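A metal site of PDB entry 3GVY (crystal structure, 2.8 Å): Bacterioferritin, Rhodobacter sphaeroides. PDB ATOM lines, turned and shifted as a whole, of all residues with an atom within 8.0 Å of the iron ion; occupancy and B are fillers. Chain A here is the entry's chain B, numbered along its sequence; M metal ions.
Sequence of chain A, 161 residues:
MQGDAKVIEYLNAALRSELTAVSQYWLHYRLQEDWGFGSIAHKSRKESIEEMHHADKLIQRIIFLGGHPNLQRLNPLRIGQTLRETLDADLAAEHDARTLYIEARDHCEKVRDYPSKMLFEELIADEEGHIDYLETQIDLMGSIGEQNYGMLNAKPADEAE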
ATOM      1  N   ALA A  14     -22.834   9.923  -8.396  1.00  0.00           N
ATOM      2  CA  ALA A  14     -21.945   9.130  -9.201  1.00  0.00           C
ATOM      3  C   ALA A  14     -20.727   8.796  -8.342  1.00  0.00           C
ATOM      4  O   ALA A  14     -20.222   7.671  -8.375  1.00  0.00           O
ATOM      5  CB  ALA A  14     -21.541   9.880 -10.400  1.00  0.00           C
ATOM      6  N   SER A  17     -21.897   5.970  -6.045  1.00  0.00           N
ATOM      7  CA  SER A  17     -22.037   4.683  -6.661  1.00  0.00           C
ATOM      8  C   SER A  17     -20.685   4.171  -7.171  1.00  0.00           C
ATOM      9  O   SER A  17     -20.555   3.008  -7.505  1.00  0.00           O
ATOM     10  CB  SER A  17     -23.100   4.725  -7.780  1.00  0.00           C
ATOM     11  OG  SER A  17     -22.600   5.325  -8.974  1.00  0.00           O
ATOM     12  N   GLU A  18     -19.687   5.059  -7.215  1.00  0.00           N
ATOM     13  CA  GLU A  18     -18.376   4.680  -7.709  1.00  0.00           C
ATOM     14  C   GLU A  18     -17.537   4.116  -6.618  1.00  0.00           C
ATOM     15  O   GLU A  18     -16.856   3.140  -6.824  1.00  0.00           O
ATOM     16  CB  GLU A  18     -17.656   5.861  -8.328  1.00  0.00           C
ATOM     17  CG  GLU A  18     -17.925   6.049  -9.811  1.00  0.00           C
ATOM     18  CD  GLU A  18     -17.546   4.825 -10.677  1.00  0.00           C
ATOM     19  OE1 GLU A  18     -16.766   3.978 -10.171  1.00  0.00           O
ATOM     20  OE2 GLU A  18     -18.006   4.707 -11.840  1.00  0.00           O
ATOM     21  N   ALA A  21     -18.803   0.686  -5.819  1.00  0.00           N
ATOM     22  CA  ALA A  21     -18.193  -0.097  -6.857  1.00  0.00           C
ATOM     23  C   ALA A  21     -16.790  -0.484  -6.410  1.00  0.00           C
ATOM     24  O   ALA A  21     -16.443  -1.680  -6.420  1.00  0.00           O
ATOM     25  CB  ALA A  21     -18.147   0.694  -8.121  1.00  0.00           C
ATOM     26  N   TYR A  25     -15.998  -4.399  -5.876  1.00  0.00           N
ATOM     27  CA  TYR A  25     -15.038  -5.050  -6.742  1.00  0.00           C
ATOM     28  C   TYR A  25     -13.844  -5.616  -5.988  1.00  0.00           C
ATOM     29  O   TYR A  25     -13.485  -6.772  -6.190  1.00  0.00           O
ATOM     30  CB  TYR A  25     -14.587  -4.107  -7.858  1.00  0.00           C
ATOM     31  CG  TYR A  25     -15.703  -3.740  -8.814  1.00  0.00           C
ATOM     32  CD1 TYR A  25     -17.016  -3.565  -8.360  1.00  0.00           C
ATOM     33  CD2 TYR A  25     -15.445  -3.531 -10.188  1.00  0.00           C
ATOM     34  CE1 TYR A  25     -18.068  -3.206  -9.232  1.00  0.00           C
ATOM     35  CE2 TYR A  25     -16.514  -3.169 -11.074  1.00  0.00           C
ATOM     36  CZ  TYR A  25     -17.815  -3.013 -10.573  1.00  0.00           C
ATOM     37  OH  TYR A  25     -18.886  -2.659 -11.384  1.00  0.00           O
ATOM     38  N   GLU A  47     -10.503  -3.806 -12.246  1.00  0.00           N
ATOM     39  CA  GLU A  47     -11.727  -3.040 -12.352  1.00  0.00           C
ATOM     40  C   GLU A  47     -12.027  -2.137 -11.135  1.00  0.00           C
ATOM     41  O   GLU A  47     -12.464  -0.970 -11.264  1.00  0.00           O
ATOM     42  CB  GLU A  47     -12.872  -4.012 -12.632  1.00  0.00           C
ATOM     43  CG  GLU A  47     -12.715  -4.718 -13.955  1.00  0.00           C
ATOM     44  CD  GLU A  47     -12.611  -3.740 -15.107  1.00  0.00           C
ATOM     45  OE1 GLU A  47     -13.590  -2.969 -15.271  1.00  0.00           O
ATOM     46  OE2 GLU A  47     -11.567  -3.713 -15.816  1.00  0.00           O
ATOM     47  N   GLU A  50      -9.997   0.756 -11.965  1.00  0.00           N
ATOM     48  CA  GLU A  50     -10.553   1.686 -12.939  1.00  0.00           C
ATOM     49  C   GLU A  50     -11.648   2.618 -12.358  1.00  0.00           C
ATOM     50  O   GLU A  50     -11.781   3.793 -12.749  1.00  0.00           O
ATOM     51  CB  GLU A  50     -10.952   1.009 -14.248  1.00  0.00           C
ATOM     52  CG  GLU A  50      -9.722   0.746 -15.183  1.00  0.00           C
ATOM     53  CD  GLU A  50     -10.027  -0.199 -16.381  1.00  0.00           C
ATOM     54  OE1 GLU A  50     -11.204  -0.207 -16.852  1.00  0.00           O
ATOM     55  OE2 GLU A  50      -9.101  -0.910 -16.859  1.00  0.00           O
ATOM     56  N   GLU A  51     -12.403   2.082 -11.397  1.00  0.00           N
ATOM     57  CA  GLU A  51     -13.346   2.896 -10.650  1.00  0.00           C
ATOM     58  C   GLU A  51     -12.599   3.878  -9.733  1.00  0.00           C
ATOM     59  O   GLU A  51     -13.016   5.024  -9.589  1.00  0.00           O
ATOM     60  CB  GLU A  51     -14.352   2.017  -9.865  1.00  0.00           C
ATOM     61  CG  GLU A  51     -15.101   0.938 -10.716  1.00  0.00           C
ATOM     62  CD  GLU A  51     -16.319   1.470 -11.511  1.00  0.00           C
ATOM     63  OE1 GLU A  51     -17.325   0.745 -11.686  1.00  0.00           O
ATOM     64  OE2 GLU A  51     -16.281   2.646 -11.967  1.00  0.00           O
ATOM     65  N   MET A  52     -11.479   3.423  -9.158  1.00  0.00           N
ATOM     66  CA  MET A  52     -10.614   4.306  -8.352  1.00  0.00           C
ATOM     67  C   MET A  52     -10.400   5.584  -9.160  1.00  0.00           C
ATOM     68  O   MET A  52     -10.425   6.689  -8.626  1.00  0.00           O
ATOM     69  CB  MET A  52      -9.256   3.663  -8.060  1.00  0.00           C
ATOM     70  CG  MET A  52      -9.235   2.567  -6.994  1.00  0.00           C
ATOM     71  SD  MET A  52      -7.987   2.527  -5.630  1.00  0.00           S
ATOM     72  CE  MET A  52      -8.668   0.871  -5.356  1.00  0.00           C
ATOM     73  N   HIS A  53     -10.245   5.413 -10.474  1.00  0.00           N
ATOM     74  CA  HIS A  53      -9.971   6.510 -11.362  1.00  0.00           C
ATOM     75  C   HIS A  53     -11.170   7.320 -11.692  1.00  0.00           C
ATOM     76  O   HIS A  53     -11.058   8.496 -12.002  1.00  0.00           O
ATOM     77  CB  HIS A  53      -9.397   6.008 -12.644  1.00  0.00           C
ATOM     78  CG  HIS A  53      -7.980   5.580 -12.509  1.00  0.00           C
ATOM     79  ND1 HIS A  53      -6.953   6.476 -12.361  1.00  0.00           N
ATOM     80  CD2 HIS A  53      -7.414   4.345 -12.456  1.00  0.00           C
ATOM     81  CE1 HIS A  53      -5.814   5.836 -12.240  1.00  0.00           C
ATOM     82  NE2 HIS A  53      -6.068   4.538 -12.291  1.00  0.00           N
ATOM     83  N   HIS A  54     -12.323   6.678 -11.669  1.00  0.00           N
ATOM     84  CA  HIS A  54     -13.535   7.412 -11.914  1.00  0.00           C
ATOM     85  C   HIS A  54     -13.820   8.287 -10.722  1.00  0.00           C
ATOM     86  O   HIS A  54     -13.965   9.510 -10.874  1.00  0.00           O
ATOM     87  CB  HIS A  54     -14.690   6.466 -12.214  1.00  0.00           C
ATOM     88  CG  HIS A  54     -14.596   5.825 -13.553  1.00  0.00           C
ATOM     89  ND1 HIS A  54     -15.371   4.745 -13.914  1.00  0.00           N
ATOM     90  CD2 HIS A  54     -13.811   6.109 -14.612  1.00  0.00           C
ATOM     91  CE1 HIS A  54     -15.069   4.393 -15.156  1.00  0.00           C
ATOM     92  NE2 HIS A  54     -14.122   5.211 -15.602  1.00  0.00           N
ATOM     93  N   ALA A  55     -13.895   7.664  -9.545  1.00  0.00           N
ATOM     94  CA  ALA A  55     -14.018   8.386  -8.288  1.00  0.00           C
ATOM     95  C   ALA A  55     -13.207   9.641  -8.335  1.00  0.00           C
ATOM     96  O   ALA A  55     -13.726  10.721  -8.137  1.00  0.00           O
ATOM     97  CB  ALA A  55     -13.545   7.510  -7.144  1.00  0.00           C
ATOM     98  N   LEU A  58     -14.400  12.340 -10.622  1.00  0.00           N
ATOM     99  CA  LEU A  58     -15.616  12.965 -10.099  1.00  0.00           C
ATOM    100  C   LEU A  58     -15.292  13.951  -9.007  1.00  0.00           C
ATOM    101  O   LEU A  58     -15.809  15.078  -9.017  1.00  0.00           O
ATOM    102  CB  LEU A  58     -16.643  11.925  -9.653  1.00  0.00           C
ATOM    103  CG  LEU A  58     -17.362  11.327 -10.865  1.00  0.00           C
ATOM    104  CD1 LEU A  58     -17.952   9.978 -10.503  1.00  0.00           C
ATOM    105  CD2 LEU A  58     -18.436  12.263 -11.438  1.00  0.00           C
ATOM    106  N   GLU A  94     -23.586  -2.400 -11.900  1.00  0.00           N
ATOM    107  CA  GLU A  94     -23.363  -1.753 -13.168  1.00  0.00           C
ATOM    108  C   GLU A  94     -24.637  -1.231 -13.818  1.00  0.00           C
ATOM    109  O   GLU A  94     -24.711  -0.027 -14.089  1.00  0.00           O
ATOM    110  CB  GLU A  94     -22.625  -2.684 -14.118  1.00  0.00           C
ATOM    111  CG  GLU A  94     -21.162  -2.854 -13.762  1.00  0.00           C
ATOM    112  CD  GLU A  94     -20.391  -1.570 -13.885  1.00  0.00           C
ATOM    113  OE1 GLU A  94     -21.016  -0.518 -14.240  1.00  0.00           O
ATOM    114  OE2 GLU A  94     -19.153  -1.612 -13.620  1.00  0.00           O
ATOM    115  N   ALA A  97     -25.673   2.070 -12.077  1.00  0.00           N
ATOM    116  CA  ALA A  97     -24.862   3.241 -12.309  1.00  0.00           C
ATOM    117  C   ALA A  97     -25.013   3.777 -13.737  1.00  0.00           C
ATOM    118  O   ALA A  97     -25.166   4.994 -13.939  1.00  0.00           O
ATOM    119  CB  ALA A  97     -23.431   2.938 -11.964  1.00  0.00           C
ATOM    120  N   ARG A  98     -24.992   2.889 -14.722  1.00  0.00           N
ATOM    121  CA  ARG A  98     -25.337   3.261 -16.088  1.00  0.00           C
ATOM    122  C   ARG A  98     -26.687   3.960 -16.138  1.00  0.00           C
ATOM    123  O   ARG A  98     -26.826   4.978 -16.798  1.00  0.00           O
ATOM    124  CB  ARG A  98     -25.355   2.060 -17.018  1.00  0.00           C
ATOM    125  CG  ARG A  98     -25.783   2.369 -18.443  1.00  0.00           C
ATOM    126  CD  ARG A  98     -26.235   1.116 -19.207  1.00  0.00           C
ATOM    127  NE  ARG A  98     -26.904   1.449 -20.471  1.00  0.00           N
ATOM    128  CZ  ARG A  98     -28.221   1.683 -20.614  1.00  0.00           C
ATOM    129  NH1 ARG A  98     -29.068   1.616 -19.585  1.00  0.00           N
ATOM    130  NH2 ARG A  98     -28.690   1.990 -21.809  1.00  0.00           N
ATOM    131  N   TYR A 101     -26.137   7.486 -14.428  1.00  0.00           N
ATOM    132  CA  TYR A 101     -25.335   8.305 -15.298  1.00  0.00           C
ATOM    133  C   TYR A 101     -26.123   8.893 -16.472  1.00  0.00           C
ATOM    134  O   TYR A 101     -25.837  10.013 -16.944  1.00  0.00           O
ATOM    135  CB  TYR A 101     -24.187   7.460 -15.867  1.00  0.00           C
ATOM    136  CG  TYR A 101     -23.148   6.988 -14.866  1.00  0.00           C
ATOM    137  CD1 TYR A 101     -23.133   7.483 -13.554  1.00  0.00           C
ATOM    138  CD2 TYR A 101     -22.150   6.088 -15.241  1.00  0.00           C
ATOM    139  CE1 TYR A 101     -22.170   7.058 -12.622  1.00  0.00           C
ATOM    140  CE2 TYR A 101     -21.172   5.672 -14.327  1.00  0.00           C
ATOM    141  CZ  TYR A 101     -21.195   6.165 -13.019  1.00  0.00           C
ATOM    142  OH  TYR A 101     -20.241   5.748 -12.103  1.00  0.00           O
ATOM    143  N   GLU A 122     -18.901   9.701 -21.192  1.00  0.00           N
ATOM    144  CA  GLU A 122     -17.746   8.820 -21.090  1.00  0.00           C
ATOM    145  C   GLU A 122     -17.960   7.718 -20.075  1.00  0.00           C
ATOM    146  O   GLU A 122     -17.622   6.575 -20.373  1.00  0.00           O
ATOM    147  CB  GLU A 122     -16.461   9.591 -20.769  1.00  0.00           C
ATOM    148  CG  GLU A 122     -15.994  10.451 -21.911  1.00  0.00           C
ATOM    149  CD  GLU A 122     -15.378   9.654 -23.063  1.00  0.00           C
ATOM    150  OE1 GLU A 122     -14.288   9.067 -22.884  1.00  0.00           O
ATOM    151  OE2 GLU A 122     -15.968   9.618 -24.168  1.00  0.00           O
ATOM    152  N   LEU A 123     -18.501   8.048 -18.902  1.00  0.00           N
ATOM    153  CA  LEU A 123     -18.691   7.034 -17.844  1.00  0.00           C
ATOM    154  C   LEU A 123     -19.620   5.897 -18.280  1.00  0.00           C
ATOM    155  O   LEU A 123     -19.443   4.726 -17.902  1.00  0.00           O
ATOM    156  CB  LEU A 123     -19.193   7.641 -16.527  1.00  0.00           C
ATOM    157  CG  LEU A 123     -18.222   8.270 -15.519  1.00  0.00           C
ATOM    158  CD1 LEU A 123     -18.999   8.567 -14.230  1.00  0.00           C
ATOM    159  CD2 LEU A 123     -16.984   7.414 -15.211  1.00  0.00           C
ATOM    160  N   ILE A 124     -20.609   6.258 -19.099  1.00  0.00           N
ATOM    161  CA  ILE A 124     -21.486   5.278 -19.678  1.00  0.00           C
ATOM    162  C   ILE A 124     -20.660   4.241 -20.429  1.00  0.00           C
ATOM    163  O   ILE A 124     -20.656   3.063 -20.063  1.00  0.00           O
ATOM    164  CB  ILE A 124     -22.521   5.925 -20.618  1.00  0.00           C
ATOM    165  CG1 ILE A 124     -23.162   7.133 -19.945  1.00  0.00           C
ATOM    166  CG2 ILE A 124     -23.543   4.907 -21.037  1.00  0.00           C
ATOM    167  CD1 ILE A 124     -24.462   7.541 -20.573  1.00  0.00           C
ATOM    168  N   ALA A 125     -19.908   4.680 -21.426  1.00  0.00           N
ATOM    169  CA  ALA A 125     -19.123   3.759 -22.258  1.00  0.00           C
ATOM    170  C   ALA A 125     -18.209   2.847 -21.458  1.00  0.00           C
ATOM    171  O   ALA A 125     -17.905   1.753 -21.903  1.00  0.00           O
ATOM    172  CB  ALA A 125     -18.338   4.513 -23.331  1.00  0.00           C
ATOM    173  N   ASP A 126     -17.780   3.274 -20.283  1.00  0.00           N
ATOM    174  CA  ASP A 126     -16.951   2.417 -19.466  1.00  0.00           C
ATOM    175  C   ASP A 126     -17.761   1.451 -18.642  1.00  0.00           C
ATOM    176  O   ASP A 126     -17.300   0.385 -18.334  1.00  0.00           O
ATOM    177  CB  ASP A 126     -16.083   3.252 -18.533  1.00  0.00           C
ATOM    178  CG  ASP A 126     -15.110   4.121 -19.277  1.00  0.00           C
ATOM    179  OD1 ASP A 126     -15.362   4.440 -20.472  1.00  0.00           O
ATOM    180  OD2 ASP A 126     -14.098   4.504 -18.653  1.00  0.00           O
ATOM    181  N   GLU A 127     -18.975   1.815 -18.255  1.00  0.00           N
ATOM    182  CA  GLU A 127     -19.799   0.845 -17.552  1.00  0.00           C
ATOM    183  C   GLU A 127     -20.411  -0.188 -18.528  1.00  0.00           C
ATOM    184  O   GLU A 127     -20.794  -1.302 -18.121  1.00  0.00           O
ATOM    185  CB  GLU A 127     -20.829   1.542 -16.683  1.00  0.00           C
ATOM    186  CG  GLU A 127     -20.173   2.559 -15.729  1.00  0.00           C
ATOM    187  CD  GLU A 127     -19.675   1.935 -14.420  1.00  0.00           C
ATOM    188  OE1 GLU A 127     -20.007   2.473 -13.321  1.00  0.00           O
ATOM    189  OE2 GLU A 127     -18.944   0.905 -14.480  1.00  0.00           O
ATOM    190  N   GLU A 128     -20.450   0.207 -19.802  1.00  0.00           N
ATOM    191  CA  GLU A 128     -20.964  -0.582 -20.894  1.00  0.00           C
ATOM    192  C   GLU A 128     -19.944  -1.616 -21.262  1.00  0.00           C
ATOM    193  O   GLU A 128     -20.248  -2.789 -21.409  1.00  0.00           O
ATOM    194  CB  GLU A 128     -21.162   0.331 -22.084  1.00  0.00           C
ATOM    195  CG  GLU A 128     -22.171   1.472 -21.873  1.00  0.00           C
ATOM    196  CD  GLU A 128     -23.487   1.314 -22.668  1.00  0.00           C
ATOM    197  OE1 GLU A 128     -23.425   0.990 -23.888  1.00  0.00           O
ATOM    198  OE2 GLU A 128     -24.574   1.542 -22.058  1.00  0.00           O
ATOM    199  N   HIS A 130     -17.949  -2.829 -19.205  1.00  0.00           N
ATOM    200  CA  HIS A 130     -17.988  -3.775 -18.102  1.00  0.00           C
ATOM    201  C   HIS A 130     -19.200  -4.695 -18.200  1.00  0.00           C
ATOM    202  O   HIS A 130     -19.129  -5.872 -17.862  1.00  0.00           O
ATOM    203  CB  HIS A 130     -17.872  -3.088 -16.741  1.00  0.00           C
ATOM    204  CG  HIS A 130     -17.371  -3.988 -15.653  1.00  0.00           C
ATOM    205  ND1 HIS A 130     -17.569  -3.727 -14.305  1.00  0.00           N
ATOM    206  CD2 HIS A 130     -16.697  -5.169 -15.717  1.00  0.00           C
ATOM    207  CE1 HIS A 130     -17.048  -4.719 -13.598  1.00  0.00           C
ATOM    208  NE2 HIS A 130     -16.497  -5.592 -14.428  1.00  0.00           N
HETATM  209 FE    FE M   1     -17.234   3.452 -13.723  1.00  0.00          FE
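CD of Glu 127 touches the iron ion, 3.0 Å away. Within 4 Å of the iron ion: Glu 18, Glu 51, His 54 and Glu 127. The nearest printed residue that does not touch the iron ion is Tyr 101 (4.1 Å).
OE2 of Glu 127 lies close to OE1 of Glu 94, 2.5 Å away. A ring nitrogen (NE2) of His 54 lies within hydrogen-bond range of the side-chain carboxylate of Asp 126, 3.1 Å away. OH of Tyr 101 sits close to OE2 of Glu 18, at 2.5 Å.
The iron ion is bound by OE2 of Glu 51, ND1 of His 54 and OE2 of Glu 18.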
